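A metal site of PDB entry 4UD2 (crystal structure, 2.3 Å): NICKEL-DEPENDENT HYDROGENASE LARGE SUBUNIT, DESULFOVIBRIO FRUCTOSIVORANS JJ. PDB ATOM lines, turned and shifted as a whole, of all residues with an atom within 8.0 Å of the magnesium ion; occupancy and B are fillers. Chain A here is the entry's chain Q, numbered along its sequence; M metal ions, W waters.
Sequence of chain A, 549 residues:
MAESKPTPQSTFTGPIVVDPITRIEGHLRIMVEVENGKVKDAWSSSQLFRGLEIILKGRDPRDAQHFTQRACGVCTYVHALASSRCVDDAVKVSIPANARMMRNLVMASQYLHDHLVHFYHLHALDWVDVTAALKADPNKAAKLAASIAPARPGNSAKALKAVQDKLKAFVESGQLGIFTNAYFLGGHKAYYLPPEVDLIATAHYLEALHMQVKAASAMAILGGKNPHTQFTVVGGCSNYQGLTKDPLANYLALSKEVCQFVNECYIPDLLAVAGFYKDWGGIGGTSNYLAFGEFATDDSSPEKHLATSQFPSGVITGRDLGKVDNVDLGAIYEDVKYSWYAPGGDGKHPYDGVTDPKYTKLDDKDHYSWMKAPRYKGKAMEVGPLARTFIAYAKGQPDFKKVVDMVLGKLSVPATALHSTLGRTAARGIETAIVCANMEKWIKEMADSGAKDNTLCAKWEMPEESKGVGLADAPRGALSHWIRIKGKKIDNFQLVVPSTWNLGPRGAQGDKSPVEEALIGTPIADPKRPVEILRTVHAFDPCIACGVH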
ATOM      1  N   PHE A  49      10.649 -20.963 -19.466  1.00  0.00           N
ATOM      2  CA  PHE A  49       9.514 -20.133 -19.029  1.00  0.00           C
ATOM      3  C   PHE A  49       9.532 -20.022 -17.524  1.00  0.00           C
ATOM      4  O   PHE A  49       9.682 -21.045 -16.839  1.00  0.00           O
ATOM      5  CB  PHE A  49       8.195 -20.778 -19.482  1.00  0.00           C
ATOM      6  CG  PHE A  49       6.967 -19.997 -19.099  1.00  0.00           C
ATOM      7  CD1 PHE A  49       6.536 -18.918 -19.859  1.00  0.00           C
ATOM      8  CD2 PHE A  49       6.262 -20.316 -17.948  1.00  0.00           C
ATOM      9  CE1 PHE A  49       5.403 -18.189 -19.488  1.00  0.00           C
ATOM     10  CE2 PHE A  49       5.134 -19.593 -17.554  1.00  0.00           C
ATOM     11  CZ  PHE A  49       4.705 -18.522 -18.325  1.00  0.00           C
ATOM     12  N   GLU A  53       4.375 -12.680 -15.328  1.00  0.00           N
ATOM     13  CA  GLU A  53       3.051 -12.062 -15.540  1.00  0.00           C
ATOM     14  C   GLU A  53       1.981 -12.773 -14.747  1.00  0.00           C
ATOM     15  O   GLU A  53       1.095 -12.141 -14.186  1.00  0.00           O
ATOM     16  CB  GLU A  53       2.709 -12.035 -17.019  1.00  0.00           C
ATOM     17  CG  GLU A  53       3.504 -11.010 -17.824  1.00  0.00           C
ATOM     18  CD  GLU A  53       3.702 -11.395 -19.288  1.00  0.00           C
ATOM     19  OE1 GLU A  53       3.502 -12.586 -19.628  1.00  0.00           O
ATOM     20  OE2 GLU A  53       4.080 -10.507 -20.088  1.00  0.00           O
ATOM     21  N   GLU A 334       0.477  -9.007 -29.574  1.00  0.00           N
ATOM     22  CA  GLU A 334       1.296 -10.223 -29.559  1.00  0.00           C
ATOM     23  C   GLU A 334       0.529 -11.433 -30.080  1.00  0.00           C
ATOM     24  O   GLU A 334      -0.640 -11.630 -29.742  1.00  0.00           O
ATOM     25  CB  GLU A 334       1.861 -10.493 -28.152  1.00  0.00           C
ATOM     26  CG  GLU A 334       2.792  -9.394 -27.636  1.00  0.00           C
ATOM     27  CD  GLU A 334       3.254  -9.600 -26.181  1.00  0.00           C
ATOM     28  OE1 GLU A 334       2.415  -9.525 -25.234  1.00  0.00           O
ATOM     29  OE2 GLU A 334       4.471  -9.820 -25.960  1.00  0.00           O
ATOM     30  N   TYR A 341       1.786 -21.565 -25.973  1.00  0.00           N
ATOM     31  CA  TYR A 341       0.672 -20.999 -25.205  1.00  0.00           C
ATOM     32  C   TYR A 341      -0.633 -21.570 -25.759  1.00  0.00           C
ATOM     33  O   TYR A 341      -0.660 -22.014 -26.883  1.00  0.00           O
ATOM     34  CB  TYR A 341       0.695 -19.458 -25.288  1.00  0.00           C
ATOM     35  CG  TYR A 341       1.937 -18.873 -24.622  1.00  0.00           C
ATOM     36  CD1 TYR A 341       2.014 -18.723 -23.217  1.00  0.00           C
ATOM     37  CD2 TYR A 341       3.049 -18.516 -25.372  1.00  0.00           C
ATOM     38  CE1 TYR A 341       3.170 -18.247 -22.610  1.00  0.00           C
ATOM     39  CE2 TYR A 341       4.196 -18.016 -24.767  1.00  0.00           C
ATOM     40  CZ  TYR A 341       4.257 -17.898 -23.405  1.00  0.00           C
ATOM     41  OH  TYR A 341       5.425 -17.442 -22.844  1.00  0.00           O
ATOM     42  N   PRO A 350      -1.335  -5.613 -25.396  1.00  0.00           N
ATOM     43  CA  PRO A 350      -0.875  -5.880 -24.041  1.00  0.00           C
ATOM     44  C   PRO A 350      -1.883  -5.594 -22.910  1.00  0.00           C
ATOM     45  O   PRO A 350      -1.962  -6.390 -21.976  1.00  0.00           O
ATOM     46  CB  PRO A 350       0.339  -4.988 -23.925  1.00  0.00           C
ATOM     47  CG  PRO A 350       0.904  -4.993 -25.286  1.00  0.00           C
ATOM     48  CD  PRO A 350      -0.299  -4.933 -26.190  1.00  0.00           C
ATOM     49  N   GLY A 353      -3.581  -8.574 -22.659  1.00  0.00           N
ATOM     50  CA  GLY A 353      -2.636  -9.679 -22.714  1.00  0.00           C
ATOM     51  C   GLY A 353      -3.079 -10.955 -22.013  1.00  0.00           C
ATOM     52  O   GLY A 353      -3.797 -10.920 -20.999  1.00  0.00           O
ATOM     53  N   VAL A 354      -2.640 -12.099 -22.543  1.00  0.00           N
ATOM     54  CA  VAL A 354      -3.020 -13.376 -21.974  1.00  0.00           C
ATOM     55  C   VAL A 354      -1.764 -14.217 -21.929  1.00  0.00           C
ATOM     56  O   VAL A 354      -1.075 -14.357 -22.948  1.00  0.00           O
ATOM     57  CB  VAL A 354      -4.125 -14.086 -22.806  1.00  0.00           C
ATOM     58  CG1 VAL A 354      -4.454 -15.483 -22.269  1.00  0.00           C
ATOM     59  CG2 VAL A 354      -5.401 -13.248 -22.843  1.00  0.00           C
ATOM     60  N   THR A 355      -1.460 -14.759 -20.753  1.00  0.00           N
ATOM     61  CA  THR A 355      -0.336 -15.662 -20.595  1.00  0.00           C
ATOM     62  C   THR A 355      -0.792 -17.023 -20.047  1.00  0.00           C
ATOM     63  O   THR A 355      -0.895 -17.224 -18.813  1.00  0.00           O
ATOM     64  CB  THR A 355       0.759 -15.031 -19.702  1.00  0.00           C
ATOM     65  OG1 THR A 355       1.126 -13.746 -20.225  1.00  0.00           O
ATOM     66  CG2 THR A 355       1.978 -15.929 -19.638  1.00  0.00           C
ATOM     67  N   TRP A 370       8.949 -20.295 -26.160  1.00  0.00           N
ATOM     68  CA  TRP A 370       8.279 -19.711 -24.987  1.00  0.00           C
ATOM     69  C   TRP A 370       8.068 -18.181 -25.100  1.00  0.00           C
ATOM     70  O   TRP A 370       7.272 -17.591 -24.332  1.00  0.00           O
ATOM     71  CB  TRP A 370       9.040 -20.033 -23.727  1.00  0.00           C
ATOM     72  CG  TRP A 370       8.854 -21.444 -23.250  1.00  0.00           C
ATOM     73  CD1 TRP A 370       9.797 -22.426 -23.230  1.00  0.00           C
ATOM     74  CD2 TRP A 370       7.647 -22.001 -22.707  1.00  0.00           C
ATOM     75  NE1 TRP A 370       9.250 -23.575 -22.697  1.00  0.00           N
ATOM     76  CE2 TRP A 370       7.940 -23.348 -22.366  1.00  0.00           C
ATOM     77  CE3 TRP A 370       6.355 -21.506 -22.467  1.00  0.00           C
ATOM     78  CZ2 TRP A 370       6.994 -24.202 -21.801  1.00  0.00           C
ATOM     79  CZ3 TRP A 370       5.390 -22.372 -21.905  1.00  0.00           C
ATOM     80  CH2 TRP A 370       5.731 -23.705 -21.574  1.00  0.00           C
ATOM     81  N   MET A 371       8.748 -17.573 -26.073  1.00  0.00           N
ATOM     82  CA  MET A 371       8.468 -16.188 -26.442  1.00  0.00           C
ATOM     83  C   MET A 371       7.185 -16.058 -27.272  1.00  0.00           C
ATOM     84  O   MET A 371       6.872 -16.923 -28.094  1.00  0.00           O
ATOM     85  CB  MET A 371       9.633 -15.608 -27.240  1.00  0.00           C
ATOM     86  CG  MET A 371      10.859 -15.311 -26.394  1.00  0.00           C
ATOM     87  SD  MET A 371      11.972 -14.198 -27.268  1.00  0.00           S
ATOM     88  CE  MET A 371      13.548 -14.608 -26.559  1.00  0.00           C
ATOM     89  N   LYS A 372       6.443 -14.958 -27.043  1.00  0.00           N
ATOM     90  CA  LYS A 372       5.287 -14.579 -27.853  1.00  0.00           C
ATOM     91  C   LYS A 372       5.854 -13.857 -29.068  1.00  0.00           C
ATOM     92  O   LYS A 372       7.058 -13.554 -29.098  1.00  0.00           O
ATOM     93  CB  LYS A 372       4.335 -13.642 -27.090  1.00  0.00           C
ATOM     94  CG  LYS A 372       3.680 -14.270 -25.867  1.00  0.00           C
ATOM     95  CD  LYS A 372       2.791 -13.289 -25.135  1.00  0.00           C
ATOM     96  CE  LYS A 372       2.066 -13.949 -23.974  1.00  0.00           C
ATOM     97  NZ  LYS A 372       1.330 -12.901 -23.200  1.00  0.00           N
ATOM     98  N   PRO A 374       5.579 -10.475 -30.898  1.00  0.00           N
ATOM     99  CA  PRO A 374       5.084  -9.094 -30.996  1.00  0.00           C
ATOM    100  C   PRO A 374       5.091  -8.599 -32.438  1.00  0.00           C
ATOM    101  O   PRO A 374       6.084  -8.761 -33.167  1.00  0.00           O
ATOM    102  CB  PRO A 374       6.083  -8.279 -30.133  1.00  0.00           C
ATOM    103  CG  PRO A 374       6.774  -9.315 -29.271  1.00  0.00           C
ATOM    104  CD  PRO A 374       6.876 -10.511 -30.176  1.00  0.00           C
ATOM    105  N   SER A 480       8.154  -2.144 -22.960  1.00  0.00           N
ATOM    106  CA  SER A 480       6.886  -1.604 -22.459  1.00  0.00           C
ATOM    107  C   SER A 480       6.224  -2.504 -21.442  1.00  0.00           C
ATOM    108  O   SER A 480       6.135  -3.714 -21.653  1.00  0.00           O
ATOM    109  CB  SER A 480       5.916  -1.281 -23.606  1.00  0.00           C
ATOM    110  OG  SER A 480       5.617  -2.432 -24.391  1.00  0.00           O
ATOM    111  N   TRP A 482       2.675  -2.972 -19.181  1.00  0.00           N
ATOM    112  CA  TRP A 482       1.297  -2.577 -19.263  1.00  0.00           C
ATOM    113  C   TRP A 482       0.546  -3.134 -18.052  1.00  0.00           C
ATOM    114  O   TRP A 482       0.571  -4.363 -17.804  1.00  0.00           O
ATOM    115  CB  TRP A 482       0.671  -3.071 -20.571  1.00  0.00           C
ATOM    116  CG  TRP A 482       1.492  -2.822 -21.815  1.00  0.00           C
ATOM    117  CD1 TRP A 482       2.630  -3.489 -22.198  1.00  0.00           C
ATOM    118  CD2 TRP A 482       1.218  -1.869 -22.864  1.00  0.00           C
ATOM    119  NE1 TRP A 482       3.076  -3.007 -23.411  1.00  0.00           N
ATOM    120  CE2 TRP A 482       2.234  -2.018 -23.845  1.00  0.00           C
ATOM    121  CE3 TRP A 482       0.203  -0.910 -23.081  1.00  0.00           C
ATOM    122  CZ2 TRP A 482       2.285  -1.225 -24.993  1.00  0.00           C
ATOM    123  CZ3 TRP A 482       0.266  -0.126 -24.228  1.00  0.00           C
ATOM    124  CH2 TRP A 482       1.293  -0.295 -25.173  1.00  0.00           C
ATOM    125  N   PHE A 493      -0.959  -7.664 -15.830  1.00  0.00           N
ATOM    126  CA  PHE A 493       0.340  -7.019 -15.957  1.00  0.00           C
ATOM    127  C   PHE A 493       1.088  -7.730 -17.060  1.00  0.00           C
ATOM    128  O   PHE A 493       1.375  -8.918 -16.937  1.00  0.00           O
ATOM    129  CB  PHE A 493       1.170  -7.097 -14.667  1.00  0.00           C
ATOM    130  CG  PHE A 493       2.237  -6.050 -14.585  1.00  0.00           C
ATOM    131  CD1 PHE A 493       3.371  -6.139 -15.370  1.00  0.00           C
ATOM    132  CD2 PHE A 493       2.087  -4.949 -13.761  1.00  0.00           C
ATOM    133  CE1 PHE A 493       4.350  -5.134 -15.337  1.00  0.00           C
ATOM    134  CE2 PHE A 493       3.058  -3.942 -13.721  1.00  0.00           C
ATOM    135  CZ  PHE A 493       4.195  -4.040 -14.518  1.00  0.00           C
ATOM    136  N   GLN A 494       1.385  -7.003 -18.142  1.00  0.00           N
ATOM    137  CA  GLN A 494       2.035  -7.632 -19.292  1.00  0.00           C
ATOM    138  C   GLN A 494       3.345  -6.955 -19.644  1.00  0.00           C
ATOM    139  O   GLN A 494       3.425  -5.715 -19.633  1.00  0.00           O
ATOM    140  CB  GLN A 494       1.121  -7.613 -20.508  1.00  0.00           C
ATOM    141  CG  GLN A 494      -0.138  -8.422 -20.315  1.00  0.00           C
ATOM    142  CD  GLN A 494       0.144  -9.900 -20.356  1.00  0.00           C
ATOM    143  OE1 GLN A 494       0.872 -10.384 -21.241  1.00  0.00           O
ATOM    144  NE2 GLN A 494      -0.402 -10.622 -19.393  1.00  0.00           N
ATOM    145  N   LEU A 495       4.363  -7.747 -19.960  1.00  0.00           N
ATOM    146  CA  LEU A 495       5.647  -7.205 -20.402  1.00  0.00           C
ATOM    147  C   LEU A 495       5.837  -7.531 -21.877  1.00  0.00           C
ATOM    148  O   LEU A 495       5.595  -8.675 -22.300  1.00  0.00           O
ATOM    149  CB  LEU A 495       6.810  -7.824 -19.611  1.00  0.00           C
ATOM    150  CG  LEU A 495       7.007  -7.569 -18.120  1.00  0.00           C
ATOM    151  CD1 LEU A 495       5.891  -8.189 -17.280  1.00  0.00           C
ATOM    152  CD2 LEU A 495       8.329  -8.187 -17.699  1.00  0.00           C
ATOM    153  N   VAL A 496       6.265  -6.535 -22.662  1.00  0.00           N
ATOM    154  CA  VAL A 496       6.616  -6.729 -24.072  1.00  0.00           C
ATOM    155  C   VAL A 496       8.030  -6.201 -24.184  1.00  0.00           C
ATOM    156  O   VAL A 496       8.245  -4.994 -24.091  1.00  0.00           O
ATOM    157  CB  VAL A 496       5.651  -6.001 -25.055  1.00  0.00           C
ATOM    158  CG1 VAL A 496       5.909  -6.412 -26.486  1.00  0.00           C
ATOM    159  CG2 VAL A 496       4.211  -6.321 -24.711  1.00  0.00           C
ATOM    160  N   VAL A 497       8.994  -7.103 -24.324  1.00  0.00           N
ATOM    161  CA  VAL A 497      10.412  -6.803 -24.136  1.00  0.00           C
ATOM    162  C   VAL A 497      11.151  -6.805 -25.491  1.00  0.00           C
ATOM    163  O   VAL A 497      10.724  -7.485 -26.428  1.00  0.00           O
ATOM    164  CB  VAL A 497      11.056  -7.782 -23.138  1.00  0.00           C
ATOM    165  CG1 VAL A 497      12.476  -7.375 -22.751  1.00  0.00           C
ATOM    166  CG2 VAL A 497      10.220  -7.868 -21.878  1.00  0.00           C
ATOM    167  N   THR A 500      11.846  -9.927 -27.106  1.00  0.00           N
ATOM    168  CA  THR A 500      10.617 -10.560 -27.595  1.00  0.00           C
ATOM    169  C   THR A 500      10.333 -10.098 -29.032  1.00  0.00           C
ATOM    170  O   THR A 500       9.901 -10.918 -29.868  1.00  0.00           O
ATOM    171  CB  THR A 500       9.379 -10.259 -26.724  1.00  0.00           C
ATOM    172  OG1 THR A 500       9.721 -10.390 -25.345  1.00  0.00           O
ATOM    173  CG2 THR A 500       8.271 -11.226 -27.061  1.00  0.00           C
ATOM    174  N   CYS A 546      14.568 -12.043 -20.399  1.00  0.00           N
ATOM    175  CA  CYS A 546      13.807 -10.839 -20.795  1.00  0.00           C
ATOM    176  C   CYS A 546      12.680 -11.228 -21.749  1.00  0.00           C
ATOM    177  O   CYS A 546      11.500 -10.943 -21.502  1.00  0.00           O
ATOM    178  CB  CYS A 546      14.728  -9.816 -21.491  1.00  0.00           C
ATOM    179  SG  CYS A 546      15.392  -8.534 -20.435  1.00  0.00           S
ATOM    180  N   GLY A 547      13.069 -11.855 -22.854  1.00  0.00           N
ATOM    181  CA  GLY A 547      12.111 -12.193 -23.905  1.00  0.00           C
ATOM    182  C   GLY A 547      10.853 -12.917 -23.441  1.00  0.00           C
ATOM    183  O   GLY A 547       9.725 -12.554 -23.821  1.00  0.00           O
ATOM    184  N   VAL A 548      11.053 -13.955 -22.624  1.00  0.00           N
ATOM    185  CA  VAL A 548       9.971 -14.810 -22.130  1.00  0.00           C
ATOM    186  C   VAL A 548       9.368 -14.322 -20.813  1.00  0.00           C
ATOM    187  O   VAL A 548       8.131 -14.381 -20.634  1.00  0.00           O
ATOM    188  CB  VAL A 548      10.492 -16.247 -21.918  1.00  0.00           C
ATOM    189  CG1 VAL A 548       9.385 -17.144 -21.442  1.00  0.00           C
ATOM    190  CG2 VAL A 548      11.126 -16.785 -23.181  1.00  0.00           C
ATOM    191  N   HIS A 549      10.231 -13.844 -19.873  1.00  0.00           N
ATOM    192  CA  HIS A 549       9.818 -13.481 -18.510  1.00  0.00           C
ATOM    193  C   HIS A 549       8.792 -14.501 -17.929  1.00  0.00           C
ATOM    194  O   HIS A 549       7.750 -14.153 -17.348  1.00  0.00           O
ATOM    195  CB  HIS A 549       9.295 -12.031 -18.468  1.00  0.00           C
ATOM    196  CG  HIS A 549       8.426 -11.638 -19.622  1.00  0.00           C
ATOM    197  ND1 HIS A 549       8.937 -11.314 -20.871  1.00  0.00           N
ATOM    198  CD2 HIS A 549       7.076 -11.560 -19.740  1.00  0.00           C
ATOM    199  CE1 HIS A 549       7.929 -11.045 -21.692  1.00  0.00           C
ATOM    200  NE2 HIS A 549       6.788 -11.169 -21.031  1.00  0.00           N
ATOM    201  OXT HIS A 549       8.992 -15.722 -18.035  1.00  0.00           O
HETATM  202 MG    MG M   1       4.813 -10.649 -22.028  1.00  0.00          MG
HETATM  203  O   HOH W   1       4.326 -12.644 -22.017  1.00  0.00           O
HETATM  204  O   HOH W   2       5.604 -10.954 -23.799  1.00  0.00           O
HETATM  205  O   HOH W   3       3.023 -10.236 -22.893  1.00  0.00           O
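The magnesium ion is bound by water W2 (2.0 Å), water W3 (2.0 Å), water W1 (2.1 Å), OE2 of Glu 53 (2.1 Å), O of Leu 495 (2.1 Å) and NE2 of His 549 (2.3 Å). The magnesium ion has six donor atoms within binding distance.
The backbone carbonyl oxygen (O) of Gly 547 lies close to a ring nitrogen (ND1) of His 549. The backbone carbonyl oxygen (O) of Cys 546 lies within hydrogen-bond range of a ring nitrogen (ND1) of His 549. OE1 of Glu 53 is in hydrogen-bond range of OG1 of Thr 355 (2.7 Å). OE2 of Glu 53 sits close to OE1 of Gln 494 (3.4 Å).
Water W3 lies within hydrogen-bond range of OE1 of Glu 334, OE1 of Gln 494 and NZ of Lys 372. Water W1 lies within hydrogen-bond range of OE1 of Glu 53 (2.5 Å) and NZ of Lys 372 (3.2 Å).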
